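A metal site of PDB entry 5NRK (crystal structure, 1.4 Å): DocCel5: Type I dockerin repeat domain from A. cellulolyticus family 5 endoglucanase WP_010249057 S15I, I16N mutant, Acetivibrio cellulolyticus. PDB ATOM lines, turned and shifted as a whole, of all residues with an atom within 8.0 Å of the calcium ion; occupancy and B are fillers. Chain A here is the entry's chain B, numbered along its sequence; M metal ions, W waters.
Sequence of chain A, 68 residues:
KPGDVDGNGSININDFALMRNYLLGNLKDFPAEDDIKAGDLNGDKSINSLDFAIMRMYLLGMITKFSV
The backbone NH (N) of Ala 32 is in hydrogen-bond range of the backbone carbonyl oxygen (O) of Val 5 (3.1 Å).
The calcium ion is bound by the side-chain carboxylate (OD1) of Asp 35, 2.4 Å away.
O of Phe 30 binds the calcium ion, 2.5 Å away.
The calcium ion is bound by the backbone carbonyl oxygen (O) of Ala 32 (2.5 Å).
Water W1 binds the calcium ion, at 2.5 Å.
The calcium ion is bound by water W2 (2.6 Å).
OD2 of Asp 29 is bound to the calcium ion, at 2.9 Å.
Residues that only touch the calcium ion: Glu 33 (3.6 Å).
Within 4 Å of the calcium ion: Asp 29, Phe 30, Ala 32, Glu 33 and Asp 35.
Along chain A the residues within 4 Å of the calcium ion span positions 29 to 35.
The nearest printed residue that does not touch the calcium ion is Pro 31 (4.4 Å).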
ATOM      1  N   VAL A   5      22.178 -10.794  -1.378  1.00  0.00           N
ATOM      2  CA  VAL A   5      22.046  -9.408  -1.808  1.00  0.00           C
ATOM      3  C   VAL A   5      21.723  -9.230  -3.279  1.00  0.00           C
ATOM      4  O   VAL A   5      21.256  -8.156  -3.653  1.00  0.00           O
ATOM      5  CB  VAL A   5      23.240  -8.544  -1.371  1.00  0.00           C
ATOM      6  CG1 VAL A   5      23.306  -8.463   0.148  1.00  0.00           C
ATOM      7  CG2 VAL A   5      24.544  -9.041  -1.954  1.00  0.00           C
ATOM      8  N   LYS A  28      25.318   1.478  -6.355  1.00  0.00           N
ATOM      9  CA  LYS A  28      24.480   2.458  -5.646  1.00  0.00           C
ATOM     10  C   LYS A  28      23.565   1.740  -4.657  1.00  0.00           C
ATOM     11  O   LYS A  28      23.259   2.257  -3.569  1.00  0.00           O
ATOM     12  CB  LYS A  28      23.643   3.288  -6.621  1.00  0.00           C
ATOM     13  CG  LYS A  28      24.431   4.134  -7.602  1.00  0.00           C
ATOM     14  CD  LYS A  28      23.521   4.758  -8.641  1.00  0.00           C
ATOM     15  CE  LYS A  28      24.278   5.779  -9.489  1.00  0.00           C
ATOM     16  NZ  LYS A  28      25.338   5.158 -10.333  1.00  0.00           N
ATOM     17  N   ASP A  29      23.141   0.554  -5.051  1.00  0.00           N
ATOM     18  CA  ASP A  29      22.391  -0.305  -4.156  1.00  0.00           C
ATOM     19  C   ASP A  29      22.566  -1.755  -4.632  1.00  0.00           C
ATOM     20  O   ASP A  29      23.439  -2.051  -5.489  1.00  0.00           O
ATOM     21  CB  ASP A  29      20.905   0.120  -4.113  1.00  0.00           C
ATOM     22  CG  ASP A  29      20.150  -0.217  -5.374  1.00  0.00           C
ATOM     23  OD1 ASP A  29      20.774  -0.355  -6.457  1.00  0.00           O
ATOM     24  OD2 ASP A  29      18.907  -0.317  -5.287  1.00  0.00           O
ATOM     25  N   PHE A  30      21.769  -2.655  -4.059  1.00  0.00           N
ATOM     26  CA  PHE A  30      21.828  -4.087  -4.354  1.00  0.00           C
ATOM     27  C   PHE A  30      20.694  -4.499  -5.278  1.00  0.00           C
ATOM     28  O   PHE A  30      19.636  -3.854  -5.292  1.00  0.00           O
ATOM     29  CB  PHE A  30      21.728  -4.882  -3.064  1.00  0.00           C
ATOM     30  CG  PHE A  30      22.924  -4.758  -2.169  1.00  0.00           C
ATOM     31  CD1 PHE A  30      24.116  -5.324  -2.513  1.00  0.00           C
ATOM     32  CD2 PHE A  30      22.846  -4.074  -0.977  1.00  0.00           C
ATOM     33  CE1 PHE A  30      25.215  -5.232  -1.707  1.00  0.00           C
ATOM     34  CE2 PHE A  30      23.953  -3.963  -0.165  1.00  0.00           C
ATOM     35  CZ  PHE A  30      25.139  -4.560  -0.528  1.00  0.00           C
ATOM     36  N   PRO A  31      20.888  -5.572  -6.055  1.00  0.00           N
ATOM     37  CA  PRO A  31      19.787  -6.031  -6.904  1.00  0.00           C
ATOM     38  C   PRO A  31      18.544  -6.524  -6.151  1.00  0.00           C
ATOM     39  O   PRO A  31      17.440  -6.411  -6.672  1.00  0.00           O
ATOM     40  CB  PRO A  31      20.417  -7.187  -7.712  1.00  0.00           C
ATOM     41  CG  PRO A  31      21.872  -6.881  -7.702  1.00  0.00           C
ATOM     42  CD  PRO A  31      22.157  -6.241  -6.375  1.00  0.00           C
ATOM     43  N   ALA A  32      18.720  -7.043  -4.934  1.00  0.00           N
ATOM     44  CA  ALA A  32      17.577  -7.424  -4.095  1.00  0.00           C
ATOM     45  C   ALA A  32      16.686  -6.202  -3.877  1.00  0.00           C
ATOM     46  O   ALA A  32      17.183  -5.106  -3.649  1.00  0.00           O
ATOM     47  CB  ALA A  32      18.072  -7.933  -2.745  1.00  0.00           C
ATOM     48  N   GLU A  33      15.366  -6.397  -3.897  1.00  0.00           N
ATOM     49  CA  GLU A  33      14.447  -5.253  -3.746  1.00  0.00           C
ATOM     50  C   GLU A  33      14.605  -4.611  -2.361  1.00  0.00           C
ATOM     51  O   GLU A  33      14.697  -3.388  -2.244  1.00  0.00           O
ATOM     52  CB  GLU A  33      12.994  -5.634  -4.005  1.00  0.00           C
ATOM     53  CG  GLU A  33      12.707  -6.023  -5.452  1.00  0.00           C
ATOM     54  CD  GLU A  33      11.289  -6.504  -5.689  1.00  0.00           C
ATOM     55  OE1 GLU A  33      10.374  -6.105  -4.931  1.00  0.00           O
ATOM     56  OE2 GLU A  33      11.082  -7.282  -6.647  1.00  0.00           O
ATOM     57  N   ASP A  34      14.734  -5.452  -1.352  1.00  0.00           N
ATOM     58  CA  ASP A  34      14.794  -4.983   0.020  1.00  0.00           C
ATOM     59  C   ASP A  34      16.259  -5.049   0.459  1.00  0.00           C
ATOM     60  O   ASP A  34      16.736  -6.070   0.953  1.00  0.00           O
ATOM     61  CB  ASP A  34      13.887  -5.840   0.920  1.00  0.00           C
ATOM     62  CG  ASP A  34      13.748  -5.273   2.325  1.00  0.00           C
ATOM     63  OD1 ASP A  34      14.647  -4.535   2.785  1.00  0.00           O
ATOM     64  OD2 ASP A  34      12.724  -5.618   2.973  1.00  0.00           O
ATOM     65  N   ASP A  35      16.962  -3.948   0.250  1.00  0.00           N
ATOM     66  CA  ASP A  35      18.389  -3.887   0.489  1.00  0.00           C
ATOM     67  C   ASP A  35      18.756  -4.172   1.942  1.00  0.00           C
ATOM     68  O   ASP A  35      19.680  -4.926   2.223  1.00  0.00           O
ATOM     69  CB  ASP A  35      18.937  -2.521   0.105  1.00  0.00           C
ATOM     70  CG  ASP A  35      18.847  -2.229  -1.356  1.00  0.00           C
ATOM     71  OD1 ASP A  35      17.713  -2.139  -1.858  1.00  0.00           O
ATOM     72  OD2 ASP A  35      19.890  -2.036  -1.975  1.00  0.00           O
ATOM     73  N   ILE A  36      18.008  -3.574   2.877  1.00  0.00           N
ATOM     74  CA  ILE A  36      18.332  -3.715   4.281  1.00  0.00           C
ATOM     75  C   ILE A  36      18.071  -5.153   4.718  1.00  0.00           C
ATOM     76  O   ILE A  36      18.890  -5.754   5.382  1.00  0.00           O
ATOM     77  CB  ILE A  36      17.555  -2.714   5.173  1.00  0.00           C
ATOM     78  CG1 ILE A  36      17.901  -1.268   4.806  1.00  0.00           C
ATOM     79  CG2 ILE A  36      17.835  -2.979   6.655  1.00  0.00           C
ATOM     80  CD1 ILE A  36      19.314  -0.829   5.044  1.00  0.00           C
ATOM     81  N   ALA A  38      18.248  -7.799   2.891  1.00  0.00           N
ATOM     82  CA  ALA A  38      19.258  -8.669   2.301  1.00  0.00           C
ATOM     83  C   ALA A  38      20.648  -8.441   2.872  1.00  0.00           C
ATOM     84  O   ALA A  38      21.418  -9.394   3.012  1.00  0.00           O
ATOM     85  CB  ALA A  38      19.280  -8.509   0.783  1.00  0.00           C
HETATM   86 CA    CA M   1      17.714  -2.696  -4.157  1.00  0.00          CA
HETATM   87  O   HOH W   1      16.727  -3.378  -6.391  1.00  0.00           O
HETATM   88  O   HOH W   2      15.491  -1.404  -3.908  1.00  0.00           O
